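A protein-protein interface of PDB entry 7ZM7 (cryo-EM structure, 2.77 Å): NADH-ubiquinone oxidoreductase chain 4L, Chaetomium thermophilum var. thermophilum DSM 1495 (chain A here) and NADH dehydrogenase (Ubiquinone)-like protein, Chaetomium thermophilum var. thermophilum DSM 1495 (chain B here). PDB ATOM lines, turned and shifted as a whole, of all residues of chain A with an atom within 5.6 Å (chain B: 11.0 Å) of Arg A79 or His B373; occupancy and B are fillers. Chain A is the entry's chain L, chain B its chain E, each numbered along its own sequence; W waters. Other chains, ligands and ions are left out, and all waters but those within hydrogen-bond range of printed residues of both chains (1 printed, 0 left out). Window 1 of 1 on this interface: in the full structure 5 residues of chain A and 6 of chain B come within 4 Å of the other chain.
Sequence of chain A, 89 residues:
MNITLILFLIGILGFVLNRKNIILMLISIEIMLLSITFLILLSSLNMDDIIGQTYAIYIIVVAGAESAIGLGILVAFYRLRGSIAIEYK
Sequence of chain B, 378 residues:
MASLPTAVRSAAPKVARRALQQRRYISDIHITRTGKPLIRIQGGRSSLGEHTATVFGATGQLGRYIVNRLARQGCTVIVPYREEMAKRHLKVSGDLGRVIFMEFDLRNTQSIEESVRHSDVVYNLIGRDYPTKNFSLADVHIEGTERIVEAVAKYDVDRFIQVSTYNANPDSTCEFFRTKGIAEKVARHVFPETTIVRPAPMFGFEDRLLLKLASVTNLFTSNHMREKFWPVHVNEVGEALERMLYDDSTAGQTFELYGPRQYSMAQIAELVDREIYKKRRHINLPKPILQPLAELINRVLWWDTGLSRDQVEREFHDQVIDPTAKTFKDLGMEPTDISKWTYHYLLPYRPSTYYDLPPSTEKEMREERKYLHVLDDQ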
ATOM      1  N   LEU A  74       5.358 -31.229 -10.208  1.00  0.00           N
ATOM      2  CA  LEU A  74       4.213 -32.099 -10.415  1.00  0.00           C
ATOM      3  C   LEU A  74       2.895 -31.351 -10.248  1.00  0.00           C
ATOM      4  O   LEU A  74       1.882 -31.747 -10.824  1.00  0.00           O
ATOM      5  CB  LEU A  74       4.278 -33.279  -9.461  1.00  0.00           C
ATOM      6  CG  LEU A  74       3.171 -34.302  -9.626  1.00  0.00           C
ATOM      7  CD1 LEU A  74       3.553 -35.328 -10.662  1.00  0.00           C
ATOM      8  CD2 LEU A  74       2.835 -34.931  -8.298  1.00  0.00           C
ATOM      9  N   VAL A  75       2.873 -30.300  -9.432  1.00  0.00           N
ATOM     10  CA  VAL A  75       1.677 -29.477  -9.332  1.00  0.00           C
ATOM     11  C   VAL A  75       1.479 -28.678 -10.606  1.00  0.00           C
ATOM     12  O   VAL A  75       0.381 -28.633 -11.163  1.00  0.00           O
ATOM     13  CB  VAL A  75       1.749 -28.550  -8.104  1.00  0.00           C
ATOM     14  CG1 VAL A  75       0.788 -27.408  -8.273  1.00  0.00           C
ATOM     15  CG2 VAL A  75       1.438 -29.303  -6.856  1.00  0.00           C
ATOM     16  N   ALA A  76       2.553 -28.072 -11.109  1.00  0.00           N
ATOM     17  CA  ALA A  76       2.486 -27.272 -12.354  1.00  0.00           C
ATOM     18  C   ALA A  76       1.972 -28.140 -13.506  1.00  0.00           C
ATOM     19  O   ALA A  76       1.157 -27.644 -14.309  1.00  0.00           O
ATOM     20  CB  ALA A  76       3.852 -26.714 -12.639  1.00  0.00           C
ATOM     21  N   PHE A  77       2.423 -29.389 -13.582  1.00  0.00           N
ATOM     22  CA  PHE A  77       1.981 -30.341 -14.629  1.00  0.00           C
ATOM     23  C   PHE A  77       0.494 -30.656 -14.452  1.00  0.00           C
ATOM     24  O   PHE A  77      -0.247 -30.541 -15.437  1.00  0.00           O
ATOM     25  CB  PHE A  77       2.898 -31.567 -14.583  1.00  0.00           C
ATOM     26  CG  PHE A  77       2.545 -32.696 -15.515  1.00  0.00           C
ATOM     27  CD1 PHE A  77       2.880 -32.641 -16.857  1.00  0.00           C
ATOM     28  CD2 PHE A  77       1.901 -33.826 -15.041  1.00  0.00           C
ATOM     29  CE1 PHE A  77       2.562 -33.684 -17.708  1.00  0.00           C
ATOM     30  CE2 PHE A  77       1.586 -34.870 -15.894  1.00  0.00           C
ATOM     31  CZ  PHE A  77       1.917 -34.797 -17.224  1.00  0.00           C
ATOM     32  N   TYR A  78       0.067 -31.020 -13.242  1.00  0.00           N
ATOM     33  CA  TYR A  78      -1.343 -31.400 -12.963  1.00  0.00           C
ATOM     34  C   TYR A  78      -2.317 -30.261 -13.289  1.00  0.00           C
ATOM     35  O   TYR A  78      -3.413 -30.568 -13.754  1.00  0.00           O
ATOM     36  CB  TYR A  78      -1.457 -31.886 -11.515  1.00  0.00           C
ATOM     37  CG  TYR A  78      -2.855 -32.178 -11.033  1.00  0.00           C
ATOM     38  CD1 TYR A  78      -3.503 -33.352 -11.373  1.00  0.00           C
ATOM     39  CD2 TYR A  78      -3.519 -31.278 -10.222  1.00  0.00           C
ATOM     40  CE1 TYR A  78      -4.789 -33.616 -10.934  1.00  0.00           C
ATOM     41  CE2 TYR A  78      -4.803 -31.527  -9.772  1.00  0.00           C
ATOM     42  CZ  TYR A  78      -5.439 -32.700 -10.128  1.00  0.00           C
ATOM     43  OH  TYR A  78      -6.701 -32.937  -9.673  1.00  0.00           O
ATOM     44  N   ARG A  79      -1.938 -29.005 -13.063  1.00  0.00           N
ATOM     45  CA  ARG A  79      -2.842 -27.849 -13.282  1.00  0.00           C
ATOM     46  C   ARG A  79      -3.307 -27.834 -14.744  1.00  0.00           C
ATOM     47  O   ARG A  79      -4.490 -27.542 -14.980  1.00  0.00           O
ATOM     48  CB  ARG A  79      -2.098 -26.545 -12.975  1.00  0.00           C
ATOM     49  CG  ARG A  79      -2.968 -25.299 -13.026  1.00  0.00           C
ATOM     50  CD  ARG A  79      -2.301 -24.100 -12.390  1.00  0.00           C
ATOM     51  NE  ARG A  79      -1.310 -23.564 -13.299  1.00  0.00           N
ATOM     52  CZ  ARG A  79      -1.499 -22.512 -14.082  1.00  0.00           C
ATOM     53  NH1 ARG A  79      -0.532 -22.116 -14.884  1.00  0.00           N
ATOM     54  NH2 ARG A  79      -2.635 -21.844 -14.043  1.00  0.00           N
ATOM     55  N   LEU A  80      -2.405 -28.129 -15.685  1.00  0.00           N
ATOM     56  CA  LEU A  80      -2.764 -28.124 -17.123  1.00  0.00           C
ATOM     57  C   LEU A  80      -3.188 -29.509 -17.618  1.00  0.00           C
ATOM     58  O   LEU A  80      -3.776 -29.575 -18.699  1.00  0.00           O
ATOM     59  CB  LEU A  80      -1.577 -27.578 -17.921  1.00  0.00           C
ATOM     60  CG  LEU A  80      -0.903 -26.347 -17.321  1.00  0.00           C
ATOM     61  CD1 LEU A  80       0.371 -26.008 -18.075  1.00  0.00           C
ATOM     62  CD2 LEU A  80      -1.847 -25.158 -17.310  1.00  0.00           C
ATOM     63  N   ARG A  81      -2.885 -30.571 -16.812  1.00  0.00           N
ATOM     64  CA  ARG A  81      -3.177 -31.936 -17.321  1.00  0.00           C
ATOM     65  C   ARG A  81      -4.484 -32.450 -16.707  1.00  0.00           C
ATOM     66  O   ARG A  81      -5.358 -32.877 -17.476  1.00  0.00           O
ATOM     67  CB  ARG A  81      -1.968 -32.856 -17.115  1.00  0.00           C
ATOM     68  CG  ARG A  81      -2.033 -34.175 -17.865  1.00  0.00           C
ATOM     69  CD  ARG A  81      -1.352 -34.114 -19.215  1.00  0.00           C
ATOM     70  NE  ARG A  81      -0.915 -35.434 -19.641  1.00  0.00           N
ATOM     71  CZ  ARG A  81      -0.396 -35.709 -20.830  1.00  0.00           C
ATOM     72  NH1 ARG A  81      -0.259 -34.750 -21.730  1.00  0.00           N
ATOM     73  NH2 ARG A  81      -0.028 -36.943 -21.121  1.00  0.00           N
ATOM     74  N   GLY A  82      -4.654 -32.371 -15.418  1.00  0.00           N
ATOM     75  CA  GLY A  82      -5.834 -32.929 -14.726  1.00  0.00           C
ATOM     76  C   GLY A  82      -5.676 -34.396 -14.437  1.00  0.00           C
ATOM     77  O   GLY A  82      -6.653 -35.011 -14.010  1.00  0.00           O
ATOM     78  N   SER B 360      -9.990 -43.858 -17.462  1.00  0.00           N
ATOM     79  CA  SER B 360     -10.704 -42.889 -18.339  1.00  0.00           C
ATOM     80  C   SER B 360     -10.456 -43.113 -19.832  1.00  0.00           C
ATOM     81  O   SER B 360      -9.435 -43.735 -20.179  1.00  0.00           O
ATOM     82  CB  SER B 360     -10.371 -41.484 -17.950  1.00  0.00           C
ATOM     83  OG  SER B 360      -8.974 -41.272 -18.044  1.00  0.00           O
ATOM     84  N   GLU B 364     -12.700 -38.139 -22.930  1.00  0.00           N
ATOM     85  CA  GLU B 364     -12.883 -37.354 -21.680  1.00  0.00           C
ATOM     86  C   GLU B 364     -11.533 -36.825 -21.190  1.00  0.00           C
ATOM     87  O   GLU B 364     -11.533 -35.807 -20.485  1.00  0.00           O
ATOM     88  CB  GLU B 364     -13.670 -38.140 -20.627  1.00  0.00           C
ATOM     89  CG  GLU B 364     -13.070 -39.484 -20.272  1.00  0.00           C
ATOM     90  CD  GLU B 364     -13.964 -40.339 -19.390  1.00  0.00           C
ATOM     91  OE1 GLU B 364     -14.887 -39.778 -18.770  1.00  0.00           O
ATOM     92  OE2 GLU B 364     -13.744 -41.564 -19.336  1.00  0.00           O
ATOM     93  N   MET B 365     -10.433 -37.482 -21.553  1.00  0.00           N
ATOM     94  CA  MET B 365      -9.086 -36.961 -21.196  1.00  0.00           C
ATOM     95  C   MET B 365      -8.921 -35.609 -21.888  1.00  0.00           C
ATOM     96  O   MET B 365      -8.311 -34.714 -21.286  1.00  0.00           O
ATOM     97  CB  MET B 365      -7.978 -37.908 -21.660  1.00  0.00           C
ATOM     98  CG  MET B 365      -7.786 -39.106 -20.754  1.00  0.00           C
ATOM     99  SD  MET B 365      -7.187 -38.639 -19.111  1.00  0.00           S
ATOM    100  CE  MET B 365      -5.585 -37.954 -19.529  1.00  0.00           C
ATOM    101  N   ARG B 366      -9.428 -35.485 -23.111  1.00  0.00           N
ATOM    102  CA  ARG B 366      -9.386 -34.198 -23.853  1.00  0.00           C
ATOM    103  C   ARG B 366     -10.230 -33.149 -23.127  1.00  0.00           C
ATOM    104  O   ARG B 366      -9.826 -31.977 -23.124  1.00  0.00           O
ATOM    105  CB  ARG B 366      -9.861 -34.401 -25.296  1.00  0.00           C
ATOM    106  CG  ARG B 366      -8.888 -35.199 -26.153  1.00  0.00           C
ATOM    107  CD  ARG B 366      -9.394 -35.433 -27.563  1.00  0.00           C
ATOM    108  NE  ARG B 366     -10.580 -36.275 -27.607  1.00  0.00           N
ATOM    109  CZ  ARG B 366     -11.188 -36.651 -28.726  1.00  0.00           C
ATOM    110  NH1 ARG B 366     -10.716 -36.260 -29.898  1.00  0.00           N
ATOM    111  NH2 ARG B 366     -12.261 -37.419 -28.674  1.00  0.00           N
ATOM    112  N   GLU B 367     -11.364 -33.549 -22.558  1.00  0.00           N
ATOM    113  CA  GLU B 367     -12.287 -32.591 -21.891  1.00  0.00           C
ATOM    114  C   GLU B 367     -11.557 -31.925 -20.726  1.00  0.00           C
ATOM    115  O   GLU B 367     -11.785 -30.725 -20.505  1.00  0.00           O
ATOM    116  CB  GLU B 367     -13.564 -33.295 -21.431  1.00  0.00           C
ATOM    117  CG  GLU B 367     -14.321 -33.965 -22.561  1.00  0.00           C
ATOM    118  CD  GLU B 367     -14.836 -33.027 -23.639  1.00  0.00           C
ATOM    119  OE1 GLU B 367     -15.282 -31.915 -23.291  1.00  0.00           O
ATOM    120  OE2 GLU B 367     -14.782 -33.408 -24.825  1.00  0.00           O
ATOM    121  N   GLU B 368     -10.645 -32.663 -20.092  1.00  0.00           N
ATOM    122  CA  GLU B 368      -9.892 -32.140 -18.928  1.00  0.00           C
ATOM    123  C   GLU B 368      -8.966 -31.006 -19.374  1.00  0.00           C
ATOM    124  O   GLU B 368      -8.571 -30.220 -18.521  1.00  0.00           O
ATOM    125  CB  GLU B 368      -9.143 -33.282 -18.242  1.00  0.00           C
ATOM    126  CG  GLU B 368     -10.020 -34.472 -17.909  1.00  0.00           C
ATOM    127  CD  GLU B 368     -11.094 -34.247 -16.857  1.00  0.00           C
ATOM    128  OE1 GLU B 368     -12.113 -34.961 -16.900  1.00  0.00           O
ATOM    129  OE2 GLU B 368     -10.904 -33.376 -15.989  1.00  0.00           O
ATOM    130  N   ARG B 369      -8.678 -30.869 -20.667  1.00  0.00           N
ATOM    131  CA  ARG B 369      -7.707 -29.817 -21.061  1.00  0.00           C
ATOM    132  C   ARG B 369      -8.437 -28.479 -21.186  1.00  0.00           C
ATOM    133  O   ARG B 369      -7.770 -27.472 -21.411  1.00  0.00           O
ATOM    134  CB  ARG B 369      -6.964 -30.197 -22.343  1.00  0.00           C
ATOM    135  CG  ARG B 369      -6.315 -31.573 -22.313  1.00  0.00           C
ATOM    136  CD  ARG B 369      -5.183 -31.712 -21.313  1.00  0.00           C
ATOM    137  NE  ARG B 369      -4.476 -32.961 -21.549  1.00  0.00           N
ATOM    138  CZ  ARG B 369      -4.770 -34.115 -20.961  1.00  0.00           C
ATOM    139  NH1 ARG B 369      -5.750 -34.179 -20.078  1.00  0.00           N
ATOM    140  NH2 ARG B 369      -4.078 -35.200 -21.256  1.00  0.00           N
ATOM    141  N   LYS B 370      -9.763 -28.474 -21.061  1.00  0.00           N
ATOM    142  CA  LYS B 370     -10.494 -27.178 -21.056  1.00  0.00           C
ATOM    143  C   LYS B 370     -10.673 -26.661 -19.635  1.00  0.00           C
ATOM    144  O   LYS B 370     -11.222 -25.576 -19.505  1.00  0.00           O
ATOM    145  CB  LYS B 370     -11.880 -27.364 -21.673  1.00  0.00           C
ATOM    146  CG  LYS B 370     -11.908 -28.191 -22.950  1.00  0.00           C
ATOM    147  CD  LYS B 370     -13.305 -28.550 -23.403  1.00  0.00           C
ATOM    148  CE  LYS B 370     -13.327 -29.273 -24.732  1.00  0.00           C
ATOM    149  NZ  LYS B 370     -12.532 -30.524 -24.691  1.00  0.00           N
ATOM    150  N   TYR B 371     -10.194 -27.379 -18.622  1.00  0.00           N
ATOM    151  CA  TYR B 371     -10.269 -26.883 -17.261  1.00  0.00           C
ATOM    152  C   TYR B 371      -8.877 -26.657 -16.700  1.00  0.00           C
ATOM    153  O   TYR B 371      -7.908 -27.284 -17.125  1.00  0.00           O
ATOM    154  CB  TYR B 371     -11.021 -27.858 -16.362  1.00  0.00           C
ATOM    155  CG  TYR B 371     -12.486 -27.949 -16.670  1.00  0.00           C
ATOM    156  CD1 TYR B 371     -12.957 -28.840 -17.613  1.00  0.00           C
ATOM    157  CD2 TYR B 371     -13.392 -27.135 -16.034  1.00  0.00           C
ATOM    158  CE1 TYR B 371     -14.282 -28.926 -17.899  1.00  0.00           C
ATOM    159  CE2 TYR B 371     -14.719 -27.217 -16.315  1.00  0.00           C
ATOM    160  CZ  TYR B 371     -15.161 -28.116 -17.249  1.00  0.00           C
ATOM    161  OH  TYR B 371     -16.497 -28.188 -17.538  1.00  0.00           O
ATOM    162  N   LEU B 372      -8.792 -25.755 -15.726  1.00  0.00           N
ATOM    163  CA  LEU B 372      -7.544 -25.622 -14.942  1.00  0.00           C
ATOM    164  C   LEU B 372      -7.830 -26.450 -13.682  1.00  0.00           C
ATOM    165  O   LEU B 372      -8.916 -26.283 -13.108  1.00  0.00           O
ATOM    166  CB  LEU B 372      -7.302 -24.140 -14.641  1.00  0.00           C
ATOM    167  CG  LEU B 372      -6.384 -23.409 -15.619  1.00  0.00           C
ATOM    168  CD1 LEU B 372      -6.213 -21.954 -15.215  1.00  0.00           C
ATOM    169  CD2 LEU B 372      -5.032 -24.096 -15.707  1.00  0.00           C
ATOM    170  N   HIS B 373      -6.927 -27.335 -13.281  1.00  0.00           N
ATOM    171  CA  HIS B 373      -7.215 -28.257 -12.154  1.00  0.00           C
ATOM    172  C   HIS B 373      -6.525 -27.767 -10.885  1.00  0.00           C
ATOM    173  O   HIS B 373      -6.565 -28.482  -9.876  1.00  0.00           O
ATOM    174  CB  HIS B 373      -6.796 -29.668 -12.575  1.00  0.00           C
ATOM    175  CG  HIS B 373      -7.424 -30.085 -13.856  1.00  0.00           C
ATOM    176  ND1 HIS B 373      -8.613 -30.776 -13.900  1.00  0.00           N
ATOM    177  CD2 HIS B 373      -7.046 -29.892 -15.135  1.00  0.00           C
ATOM    178  CE1 HIS B 373      -8.936 -31.007 -15.153  1.00  0.00           C
ATOM    179  NE2 HIS B 373      -7.990 -30.478 -15.923  1.00  0.00           N
ATOM    180  N   VAL B 374      -5.935 -26.579 -10.950  1.00  0.00           N
ATOM    181  CA  VAL B 374      -5.297 -25.974  -9.752  1.00  0.00           C
ATOM    182  C   VAL B 374      -5.708 -24.512  -9.675  1.00  0.00           C
ATOM    183  O   VAL B 374      -5.902 -23.923 -10.735  1.00  0.00           O
ATOM    184  CB  VAL B 374      -3.763 -26.159  -9.731  1.00  0.00           C
ATOM    185  CG1 VAL B 374      -3.081 -25.351  -8.637  1.00  0.00           C
ATOM    186  CG2 VAL B 374      -3.370 -27.622  -9.629  1.00  0.00           C
ATOM    187  N   LEU B 375      -5.928 -23.995  -8.474  1.00  0.00           N
ATOM    188  CA  LEU B 375      -6.195 -22.577  -8.261  1.00  0.00           C
ATOM    189  C   LEU B 375      -4.915 -21.910  -7.794  1.00  0.00           C
ATOM    190  O   LEU B 375      -4.566 -21.970  -6.618  1.00  0.00           O
ATOM    191  CB  LEU B 375      -7.320 -22.395  -7.254  1.00  0.00           C
ATOM    192  CG  LEU B 375      -8.652 -22.883  -7.785  1.00  0.00           C
ATOM    193  CD1 LEU B 375      -9.658 -22.876  -6.691  1.00  0.00           C
ATOM    194  CD2 LEU B 375      -9.094 -22.002  -8.917  1.00  0.00           C
ATOM    195  N   ASP B 376      -4.225 -21.241  -8.713  1.00  0.00           N
ATOM    196  CA  ASP B 376      -2.916 -20.675  -8.427  1.00  0.00           C
ATOM    197  C   ASP B 376      -2.974 -19.329  -7.717  1.00  0.00           C
ATOM    198  O   ASP B 376      -1.925 -18.816  -7.327  1.00  0.00           O
ATOM    199  CB  ASP B 376      -2.112 -20.535  -9.714  1.00  0.00           C
ATOM    200  CG  ASP B 376      -2.851 -19.772 -10.786  1.00  0.00           C
ATOM    201  OD1 ASP B 376      -4.049 -19.472 -10.599  1.00  0.00           O
ATOM    202  OD2 ASP B 376      -2.233 -19.467 -11.824  1.00  0.00           O
ATOM    203  N   ASP B 377      -4.148 -18.752  -7.535  1.00  0.00           N
ATOM    204  CA  ASP B 377      -4.284 -17.494  -6.822  1.00  0.00           C
ATOM    205  C   ASP B 377      -4.989 -17.644  -5.486  1.00  0.00           C
ATOM    206  O   ASP B 377      -5.232 -16.642  -4.811  1.00  0.00           O
ATOM    207  CB  ASP B 377      -4.997 -16.465  -7.701  1.00  0.00           C
ATOM    208  CG  ASP B 377      -6.419 -16.857  -8.030  1.00  0.00           C
ATOM    209  OD1 ASP B 377      -6.903 -17.890  -7.520  1.00  0.00           O
ATOM    210  OD2 ASP B 377      -7.059 -16.121  -8.810  1.00  0.00           O
ATOM    211  N   GLN B 378      -5.302 -18.870  -5.087  1.00  0.00           N
ATOM    212  CA  GLN B 378      -5.899 -19.147  -3.796  1.00  0.00           C
ATOM    213  C   GLN B 378      -5.045 -20.129  -3.014  1.00  0.00           C
ATOM    214  O   GLN B 378      -4.598 -21.136  -3.548  1.00  0.00           O
ATOM    215  CB  GLN B 378      -7.314 -19.693  -3.964  1.00  0.00           C
ATOM    216  CG  GLN B 378      -8.205 -18.809  -4.816  1.00  0.00           C
ATOM    217  CD  GLN B 378      -9.672 -18.985  -4.505  1.00  0.00           C
ATOM    218  OE1 GLN B 378     -10.060 -19.149  -3.346  1.00  0.00           O
ATOM    219  NE2 GLN B 378     -10.502 -18.955  -5.543  1.00  0.00           N
HETATM  220  O   HOH W   1      -5.019 -21.899 -11.898  1.00  0.00           O
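The guanidinium group of Arg B369 is in hydrogen-bond range of the backbone carbonyl oxygen of Arg A81, at 2.9 Å.
The side-chain carboxylate (OD2) of Asp B376 is in salt-bridge range of the guanidinium group (NH2) of Arg A79 (3.3 Å).
The backbone NH (N) of His B373 sits at hydrogen-bond distance from the backbone carbonyl oxygen (O) of Arg A79 (3.0 Å).
NH1 of Arg B369 is in hydrogen-bond range of O of Met B365 (2.9 Å).
NE2 of His B373 sits at hydrogen-bond distance from O of Glu B368 (2.7 Å).
O of Tyr B371 lies close to NE2 of His B373.
Among the printed residues, pairs that only touch across the chains: Tyr A78 with His B373 (3.5 Å), Tyr A78 with Val B374 (3.7 Å), Arg A79 with Leu B372 (3.6 Å), Arg A79 with Val B374 (3.5 Å), Leu A80 with Arg B369 (3.7 Å), Leu A80 with Leu B372 (3.7 Å), Arg A81 with Glu B368 (3.9 Å), Arg A81 with His B373 (3.9 Å) and Gly A82 with His B373 (3.3 Å).
Arg A79 touches four residues of chain B.
His B373 touches just these residues of chain A: Tyr A78, Arg A79, Arg A81 and Gly A82.
No residue of chain B comes within 4 Å of Ala A76.
Leu A80 touches just these residues of chain B: Arg B369 (3.7 Å) and Leu B372 (3.7 Å).
Gly A82 touches just one residue of chain B: His B373 (3.3 Å).
Printed residues of chain A within 4 Å of Glu B368: Arg A81 (3.9 Å).
Of the printed residues of chain A, Val B374 touches Tyr A78 (3.7 Å) and Arg A79 (3.5 Å).
Printed residues of chain A within 4 Å of Arg B369: Leu A80 (3.7 Å) and Arg A81 (2.9 Å).
Of the printed residues of chain B, Arg A81 touches Glu B368, Arg B369 and His B373.
Of the printed residues of chain A, Asp B376 touches Arg A79 (3.3 Å).
Asp B377 touches none of the printed residues of chain A.
The nearest residue of chain B that does not touch Arg A79 is Tyr B371 (4.04 Å).
Printed residues of chain B that touch a printed residue of chain A: Glu B368, Arg B369, Leu B372, His B373, Val B374 and Asp B376.
Hydrophobic or aromatic side chains of chain B within 4 Å of the printed part of chain A: Leu B372, His B373 and Val B374.
Of the 9 printed residues of chain A, 5 touch a printed residue of chain B.
Printed residues of chain A that touch a printed residue of chain B: Tyr A78, Arg A79, Leu A80, Arg A81 and Gly A82.
Among the printed residues, 12 pairs touch across the chains.
Among the printed residues, Asp or Glu carboxylates within 4 Å of a Lys or Arg side-chain nitrogen of the other chain: Arg A79 with Asp B376 (3.3 Å).
Water W1 lies within hydrogen-bond range of O of Val B374, OD1 of Asp B376 and NH2 of Arg A79.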
